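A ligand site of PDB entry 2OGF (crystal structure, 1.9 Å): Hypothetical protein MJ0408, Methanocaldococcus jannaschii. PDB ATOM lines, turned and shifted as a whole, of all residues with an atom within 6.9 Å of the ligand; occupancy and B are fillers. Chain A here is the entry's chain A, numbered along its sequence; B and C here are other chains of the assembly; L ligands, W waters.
The backbone carbonyl oxygen of Pro 113 lies close to a nitrogen (N1) of the ligand (2.7 Å).
N3 of the ligand is in hydrogen-bond range of OE1 of Glu 26 of chain B (2.7 Å).
N of Met 115 is in hydrogen-bond range of N5 of the ligand (3.0 Å).
The backbone carbonyl oxygen of Met 115 lies within hydrogen-bond range of a nitrogen (N4) of the ligand (2.9 Å).
N2 of the ligand sits at hydrogen-bond distance from OH of Tyr 112 (3.2 Å).
Merely in contact with the ligand: Phe 35, Leu 114, Phe 10 of chain B, Phe 14 of chain B, Phe 25 of chain B, Ile 29 of chain B and Pro 63 of chain B.
Along chain A the residues within 4 Å of the ligand span positions 35 to 115.
The nearest printed residue that does not touch the ligand is Gln 62 of chain B (4.1 Å).
O of Glu 26 of chain B sits at hydrogen-bond distance from OG1 of Thr 30 of chain B.
The side-chain hydroxyl (OH) of Tyr 112 is in hydrogen-bond range of the side-chain hydroxyl (OH) of Tyr 79 of chain C, 2.6 Å away.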
ATOM      1  N   GLY A  32     -13.227 -14.129  21.279  1.00  0.00           N
ATOM      2  CA  GLY A  32     -11.925 -14.817  21.448  1.00  0.00           C
ATOM      3  C   GLY A  32     -11.484 -15.471  20.142  1.00  0.00           C
ATOM      4  O   GLY A  32     -10.331 -15.377  19.751  1.00  0.00           O
ATOM      5  N   PHE A  35     -10.352 -12.647  17.525  1.00  0.00           N
ATOM      6  CA  PHE A  35      -9.066 -12.106  17.914  1.00  0.00           C
ATOM      7  C   PHE A  35      -7.951 -13.064  17.498  1.00  0.00           C
ATOM      8  O   PHE A  35      -7.047 -12.690  16.739  1.00  0.00           O
ATOM      9  CB  PHE A  35      -9.092 -11.890  19.432  1.00  0.00           C
ATOM     10  CG  PHE A  35      -7.882 -11.179  20.010  1.00  0.00           C
ATOM     11  CD1 PHE A  35      -7.971  -9.844  20.408  1.00  0.00           C
ATOM     12  CD2 PHE A  35      -6.677 -11.852  20.212  1.00  0.00           C
ATOM     13  CE1 PHE A  35      -6.880  -9.194  20.977  1.00  0.00           C
ATOM     14  CE2 PHE A  35      -5.590 -11.217  20.784  1.00  0.00           C
ATOM     15  CZ  PHE A  35      -5.692  -9.883  21.162  1.00  0.00           C
ATOM     16  N   HIS A  36      -8.013 -14.307  17.965  1.00  0.00           N
ATOM     17  CA  HIS A  36      -6.909 -15.251  17.720  1.00  0.00           C
ATOM     18  C   HIS A  36      -6.823 -15.772  16.284  1.00  0.00           C
ATOM     19  O   HIS A  36      -5.735 -16.086  15.785  1.00  0.00           O
ATOM     20  CB  HIS A  36      -6.916 -16.344  18.783  1.00  0.00           C
ATOM     21  CG  HIS A  36      -6.608 -15.807  20.147  1.00  0.00           C
ATOM     22  ND1 HIS A  36      -5.340 -15.823  20.684  1.00  0.00           N
ATOM     23  CD2 HIS A  36      -7.376 -15.103  21.012  1.00  0.00           C
ATOM     24  CE1 HIS A  36      -5.364 -15.220  21.856  1.00  0.00           C
ATOM     25  NE2 HIS A  36      -6.588 -14.757  22.069  1.00  0.00           N
ATOM     26  N   GLY A  84      -4.144  -7.079  18.153  1.00  0.00           N
ATOM     27  CA  GLY A  84      -5.416  -7.030  18.894  1.00  0.00           C
ATOM     28  C   GLY A  84      -5.862  -5.623  19.310  1.00  0.00           C
ATOM     29  O   GLY A  84      -7.067  -5.358  19.385  1.00  0.00           O
ATOM     30  N   LEU A 104     -15.496  -5.404  21.568  1.00  0.00           N
ATOM     31  CA  LEU A 104     -14.033  -5.500  21.652  1.00  0.00           C
ATOM     32  C   LEU A 104     -13.431  -4.154  21.259  1.00  0.00           C
ATOM     33  O   LEU A 104     -13.660  -3.669  20.131  1.00  0.00           O
ATOM     34  CB  LEU A 104     -13.477  -6.628  20.780  1.00  0.00           C
ATOM     35  CG  LEU A 104     -11.937  -6.616  20.608  1.00  0.00           C
ATOM     36  CD1 LEU A 104     -11.169  -6.718  21.952  1.00  0.00           C
ATOM     37  CD2 LEU A 104     -11.481  -7.698  19.619  1.00  0.00           C
ATOM     38  N   TYR A 112      -5.072  -2.412  27.098  1.00  0.00           N
ATOM     39  CA  TYR A 112      -5.631  -3.758  26.926  1.00  0.00           C
ATOM     40  C   TYR A 112      -6.724  -3.756  25.876  1.00  0.00           C
ATOM     41  O   TYR A 112      -7.584  -2.862  25.882  1.00  0.00           O
ATOM     42  CB  TYR A 112      -6.172  -4.304  28.262  1.00  0.00           C
ATOM     43  CG  TYR A 112      -6.350  -5.815  28.311  1.00  0.00           C
ATOM     44  CD1 TYR A 112      -5.245  -6.668  28.360  1.00  0.00           C
ATOM     45  CD2 TYR A 112      -7.622  -6.385  28.303  1.00  0.00           C
ATOM     46  CE1 TYR A 112      -5.414  -8.055  28.400  1.00  0.00           C
ATOM     47  CE2 TYR A 112      -7.800  -7.791  28.354  1.00  0.00           C
ATOM     48  CZ  TYR A 112      -6.693  -8.604  28.395  1.00  0.00           C
ATOM     49  OH  TYR A 112      -6.849  -9.993  28.442  1.00  0.00           O
ATOM     50  N   PRO A 113      -6.708  -4.750  24.957  1.00  0.00           N
ATOM     51  CA  PRO A 113      -7.860  -4.905  24.070  1.00  0.00           C
ATOM     52  C   PRO A 113      -8.970  -5.648  24.810  1.00  0.00           C
ATOM     53  O   PRO A 113      -8.984  -6.878  24.868  1.00  0.00           O
ATOM     54  CB  PRO A 113      -7.290  -5.722  22.893  1.00  0.00           C
ATOM     55  CG  PRO A 113      -6.065  -6.388  23.417  1.00  0.00           C
ATOM     56  CD  PRO A 113      -5.632  -5.733  24.693  1.00  0.00           C
ATOM     57  N   LEU A 114      -9.903  -4.897  25.383  1.00  0.00           N
ATOM     58  CA  LEU A 114     -10.857  -5.488  26.300  1.00  0.00           C
ATOM     59  C   LEU A 114     -12.116  -6.005  25.618  1.00  0.00           C
ATOM     60  O   LEU A 114     -12.722  -5.296  24.798  1.00  0.00           O
ATOM     61  CB  LEU A 114     -11.265  -4.449  27.352  1.00  0.00           C
ATOM     62  CG  LEU A 114     -12.274  -4.881  28.432  1.00  0.00           C
ATOM     63  CD1 LEU A 114     -11.611  -5.863  29.392  1.00  0.00           C
ATOM     64  CD2 LEU A 114     -12.773  -3.668  29.198  1.00  0.00           C
ATOM     65  N   MET A 115     -12.530  -7.225  25.989  1.00  0.00           N
ATOM     66  CA  MET A 115     -13.830  -7.769  25.567  1.00  0.00           C
ATOM     67  C   MET A 115     -14.833  -7.641  26.700  1.00  0.00           C
ATOM     68  O   MET A 115     -14.527  -7.985  27.817  1.00  0.00           O
ATOM     69  CB  MET A 115     -13.684  -9.234  25.203  1.00  0.00           C
ATOM     70  CG  MET A 115     -12.749  -9.462  24.029  1.00  0.00           C
ATOM     71  SD  MET A 115     -12.140 -11.285  23.888  1.00  0.00           S
ATOM     72  CE  MET A 115     -10.858 -10.933  22.466  1.00  0.00           C
ATOM     73  N   TYR A 116     -16.030  -7.144  26.400  1.00  0.00           N
ATOM     74  CA  TYR A 116     -17.036  -6.936  27.475  1.00  0.00           C
ATOM     75  C   TYR A 116     -18.463  -6.897  26.923  1.00  0.00           C
ATOM     76  O   TYR A 116     -18.670  -6.886  25.716  1.00  0.00           O
ATOM     77  CB  TYR A 116     -16.724  -5.691  28.331  1.00  0.00           C
ATOM     78  CG  TYR A 116     -16.820  -4.338  27.623  1.00  0.00           C
ATOM     79  CD1 TYR A 116     -17.984  -3.564  27.731  1.00  0.00           C
ATOM     80  CD2 TYR A 116     -15.749  -3.823  26.884  1.00  0.00           C
ATOM     81  CE1 TYR A 116     -18.074  -2.313  27.099  1.00  0.00           C
ATOM     82  CE2 TYR A 116     -15.833  -2.579  26.254  1.00  0.00           C
ATOM     83  CZ  TYR A 116     -17.000  -1.833  26.374  1.00  0.00           C
ATOM     84  OH  TYR A 116     -17.083  -0.602  25.739  1.00  0.00           O
ATOM     85  N   PHE B  10     -10.566  -2.363  34.600  1.00  0.00           N
ATOM     86  CA  PHE B  10     -11.071  -3.613  34.018  1.00  0.00           C
ATOM     87  C   PHE B  10     -12.427  -3.959  34.658  1.00  0.00           C
ATOM     88  O   PHE B  10     -13.430  -4.124  33.957  1.00  0.00           O
ATOM     89  CB  PHE B  10     -10.048  -4.749  34.218  1.00  0.00           C
ATOM     90  CG  PHE B  10     -10.437  -6.066  33.583  1.00  0.00           C
ATOM     91  CD1 PHE B  10      -9.826  -6.498  32.403  1.00  0.00           C
ATOM     92  CD2 PHE B  10     -11.370  -6.915  34.194  1.00  0.00           C
ATOM     93  CE1 PHE B  10     -10.170  -7.720  31.819  1.00  0.00           C
ATOM     94  CE2 PHE B  10     -11.713  -8.161  33.614  1.00  0.00           C
ATOM     95  CZ  PHE B  10     -11.105  -8.557  32.421  1.00  0.00           C
ATOM     96  N   PHE B  14     -17.587  -4.653  33.956  1.00  0.00           N
ATOM     97  CA  PHE B  14     -18.340  -5.894  34.211  1.00  0.00           C
ATOM     98  C   PHE B  14     -19.364  -5.811  35.339  1.00  0.00           C
ATOM     99  O   PHE B  14     -19.856  -6.833  35.823  1.00  0.00           O
ATOM    100  CB  PHE B  14     -17.377  -7.079  34.417  1.00  0.00           C
ATOM    101  CG  PHE B  14     -16.509  -7.324  33.243  1.00  0.00           C
ATOM    102  CD1 PHE B  14     -16.991  -8.024  32.131  1.00  0.00           C
ATOM    103  CD2 PHE B  14     -15.217  -6.784  33.191  1.00  0.00           C
ATOM    104  CE1 PHE B  14     -16.198  -8.220  31.003  1.00  0.00           C
ATOM    105  CE2 PHE B  14     -14.412  -6.982  32.070  1.00  0.00           C
ATOM    106  CZ  PHE B  14     -14.914  -7.697  30.977  1.00  0.00           C
ATOM    107  N   PHE B  25     -18.738 -16.002  30.338  1.00  0.00           N
ATOM    108  CA  PHE B  25     -18.205 -15.080  29.337  1.00  0.00           C
ATOM    109  C   PHE B  25     -16.691 -15.281  29.192  1.00  0.00           C
ATOM    110  O   PHE B  25     -16.186 -15.491  28.079  1.00  0.00           O
ATOM    111  CB  PHE B  25     -18.546 -13.609  29.669  1.00  0.00           C
ATOM    112  CG  PHE B  25     -17.879 -12.591  28.748  1.00  0.00           C
ATOM    113  CD1 PHE B  25     -18.163 -12.562  27.378  1.00  0.00           C
ATOM    114  CD2 PHE B  25     -16.983 -11.665  29.264  1.00  0.00           C
ATOM    115  CE1 PHE B  25     -17.551 -11.607  26.523  1.00  0.00           C
ATOM    116  CE2 PHE B  25     -16.364 -10.702  28.429  1.00  0.00           C
ATOM    117  CZ  PHE B  25     -16.653 -10.676  27.067  1.00  0.00           C
ATOM    118  N   GLU B  26     -15.988 -15.243  30.326  1.00  0.00           N
ATOM    119  CA  GLU B  26     -14.541 -15.438  30.351  1.00  0.00           C
ATOM    120  C   GLU B  26     -14.125 -16.828  29.862  1.00  0.00           C
ATOM    121  O   GLU B  26     -13.071 -16.979  29.220  1.00  0.00           O
ATOM    122  CB  GLU B  26     -13.985 -15.211  31.763  1.00  0.00           C
ATOM    123  CG  GLU B  26     -13.996 -13.738  32.224  1.00  0.00           C
ATOM    124  CD  GLU B  26     -13.170 -12.792  31.349  1.00  0.00           C
ATOM    125  OE1 GLU B  26     -12.378 -13.277  30.506  1.00  0.00           O
ATOM    126  OE2 GLU B  26     -13.325 -11.558  31.497  1.00  0.00           O
ATOM    127  N   ILE B  29     -14.434 -16.944  26.033  1.00  0.00           N
ATOM    128  CA  ILE B  29     -13.290 -16.252  25.393  1.00  0.00           C
ATOM    129  C   ILE B  29     -12.095 -17.184  25.270  1.00  0.00           C
ATOM    130  O   ILE B  29     -11.481 -17.311  24.206  1.00  0.00           O
ATOM    131  CB  ILE B  29     -12.885 -14.945  26.145  1.00  0.00           C
ATOM    132  CG1 ILE B  29     -13.987 -13.869  26.083  1.00  0.00           C
ATOM    133  CG2 ILE B  29     -11.478 -14.409  25.632  1.00  0.00           C
ATOM    134  CD1 ILE B  29     -13.702 -12.635  27.030  1.00  0.00           C
ATOM    135  N   THR B  30     -11.781 -17.849  26.382  1.00  0.00           N
ATOM    136  CA  THR B  30     -10.584 -18.675  26.448  1.00  0.00           C
ATOM    137  C   THR B  30     -10.681 -19.906  25.531  1.00  0.00           C
ATOM    138  O   THR B  30      -9.707 -20.249  24.829  1.00  0.00           O
ATOM    139  CB  THR B  30     -10.222 -18.977  27.936  1.00  0.00           C
ATOM    140  OG1 THR B  30      -9.757 -17.754  28.569  1.00  0.00           O
ATOM    141  CG2 THR B  30      -9.162 -20.069  28.039  1.00  0.00           C
ATOM    142  N   ALA B  33     -10.534 -18.598  21.938  1.00  0.00           N
ATOM    143  CA  ALA B  33      -9.123 -18.186  21.751  1.00  0.00           C
ATOM    144  C   ALA B  33      -8.194 -19.379  21.514  1.00  0.00           C
ATOM    145  O   ALA B  33      -7.399 -19.365  20.578  1.00  0.00           O
ATOM    146  CB  ALA B  33      -8.622 -17.317  22.938  1.00  0.00           C
ATOM    147  N   GLN B  62      -4.659 -15.874  30.553  1.00  0.00           N
ATOM    148  CA  GLN B  62      -5.838 -15.060  30.272  1.00  0.00           C
ATOM    149  C   GLN B  62      -6.661 -14.690  31.521  1.00  0.00           C
ATOM    150  O   GLN B  62      -6.632 -15.411  32.511  1.00  0.00           O
ATOM    151  CB  GLN B  62      -6.713 -15.714  29.207  1.00  0.00           C
ATOM    152  CG  GLN B  62      -6.054 -15.691  27.809  1.00  0.00           C
ATOM    153  CD  GLN B  62      -7.052 -15.829  26.677  1.00  0.00           C
ATOM    154  OE1 GLN B  62      -6.863 -15.296  25.577  1.00  0.00           O
ATOM    155  NE2 GLN B  62      -8.101 -16.571  26.938  1.00  0.00           N
ATOM    156  N   PRO B  63      -7.370 -13.562  31.473  1.00  0.00           N
ATOM    157  CA  PRO B  63      -8.240 -13.204  32.626  1.00  0.00           C
ATOM    158  C   PRO B  63      -9.060 -14.356  33.193  1.00  0.00           C
ATOM    159  O   PRO B  63      -9.719 -15.089  32.452  1.00  0.00           O
ATOM    160  CB  PRO B  63      -9.128 -12.094  32.068  1.00  0.00           C
ATOM    161  CG  PRO B  63      -8.184 -11.387  31.115  1.00  0.00           C
ATOM    162  CD  PRO B  63      -7.376 -12.502  30.439  1.00  0.00           C
ATOM    163  N   CYS B  64      -8.944 -14.529  34.530  1.00  0.00           N
ATOM    164  CA  CYS B  64      -9.841 -15.363  35.316  1.00  0.00           C
ATOM    165  C   CYS B  64      -9.676 -16.872  35.097  1.00  0.00           C
ATOM    166  O   CYS B  64     -10.496 -17.659  35.567  1.00  0.00           O
ATOM    167  CB  CYS B  64     -11.314 -14.951  35.123  1.00  0.00           C
ATOM    168  SG  CYS B  64     -11.680 -13.185  35.279  1.00  0.00           S
ATOM    169  N   VAL B  65      -8.617 -17.276  34.387  1.00  0.00           N
ATOM    170  CA  VAL B  65      -8.367 -18.700  34.189  1.00  0.00           C
ATOM    171  C   VAL B  65      -7.767 -19.288  35.469  1.00  0.00           C
ATOM    172  O   VAL B  65      -6.683 -18.883  35.904  1.00  0.00           O
ATOM    173  CB  VAL B  65      -7.473 -18.996  32.951  1.00  0.00           C
ATOM    174  CG1 VAL B  65      -7.177 -20.485  32.855  1.00  0.00           C
ATOM    175  CG2 VAL B  65      -8.161 -18.507  31.666  1.00  0.00           C
ATOM    176  N   TYR C  79       1.454 -10.741  30.958  1.00  0.00           N
ATOM    177  CA  TYR C  79       1.378 -11.391  29.657  1.00  0.00           C
ATOM    178  C   TYR C  79       1.072 -10.380  28.545  1.00  0.00           C
ATOM    179  O   TYR C  79       0.448  -9.327  28.779  1.00  0.00           O
ATOM    180  CB  TYR C  79       0.397 -12.568  29.648  1.00  0.00           C
ATOM    181  CG  TYR C  79      -0.990 -12.256  29.137  1.00  0.00           C
ATOM    182  CD1 TYR C  79      -1.269 -12.326  27.770  1.00  0.00           C
ATOM    183  CD2 TYR C  79      -2.031 -11.933  30.012  1.00  0.00           C
ATOM    184  CE1 TYR C  79      -2.549 -12.040  27.277  1.00  0.00           C
ATOM    185  CE2 TYR C  79      -3.297 -11.658  29.549  1.00  0.00           C
ATOM    186  CZ  TYR C  79      -3.547 -11.718  28.179  1.00  0.00           C
ATOM    187  OH  TYR C  79      -4.800 -11.444  27.723  1.00  0.00           O
ATOM    188  N   SER C  81       0.097 -10.523  24.038  1.00  0.00           N
ATOM    189  CA  SER C  81      -0.065 -11.335  22.845  1.00  0.00           C
ATOM    190  C   SER C  81       1.294 -11.384  22.156  1.00  0.00           C
ATOM    191  O   SER C  81       1.908 -10.347  21.913  1.00  0.00           O
ATOM    192  CB  SER C  81      -1.115 -10.734  21.910  1.00  0.00           C
ATOM    193  OG  SER C  81      -2.331 -10.527  22.610  1.00  0.00           O
HETATM  194  N1  LIG L   1      -9.550  -9.304  25.851  1.00  0.00           N
HETATM  195  C1  LIG L   1      -8.665 -10.239  25.475  1.00  0.00           C
HETATM  196  N2  LIG L   1      -8.646 -11.412  26.155  1.00  0.00           N
HETATM  197  C2  LIG L   1      -9.615 -11.246  27.076  1.00  0.00           C
HETATM  198  C3  LIG L   1     -10.218 -12.045  28.168  1.00  0.00           C
HETATM  199  O1  LIG L   1      -9.849 -13.190  28.443  1.00  0.00           O
HETATM  200  N3  LIG L   1     -11.207 -11.454  28.867  1.00  0.00           N
HETATM  201  C4  LIG L   1     -11.686 -10.203  28.601  1.00  0.00           C
HETATM  202  N4  LIG L   1     -12.696  -9.715  29.336  1.00  0.00           N
HETATM  203  N5  LIG L   1     -11.179  -9.402  27.624  1.00  0.00           N
HETATM  204  C5  LIG L   1     -10.182  -9.903  26.864  1.00  0.00           C
HETATM  205  O2  LIG L   1      -7.862 -10.000  24.518  1.00  0.00           O
HETATM  206  O   HOH W   1     -10.608 -15.433  29.758  1.00  0.00           O
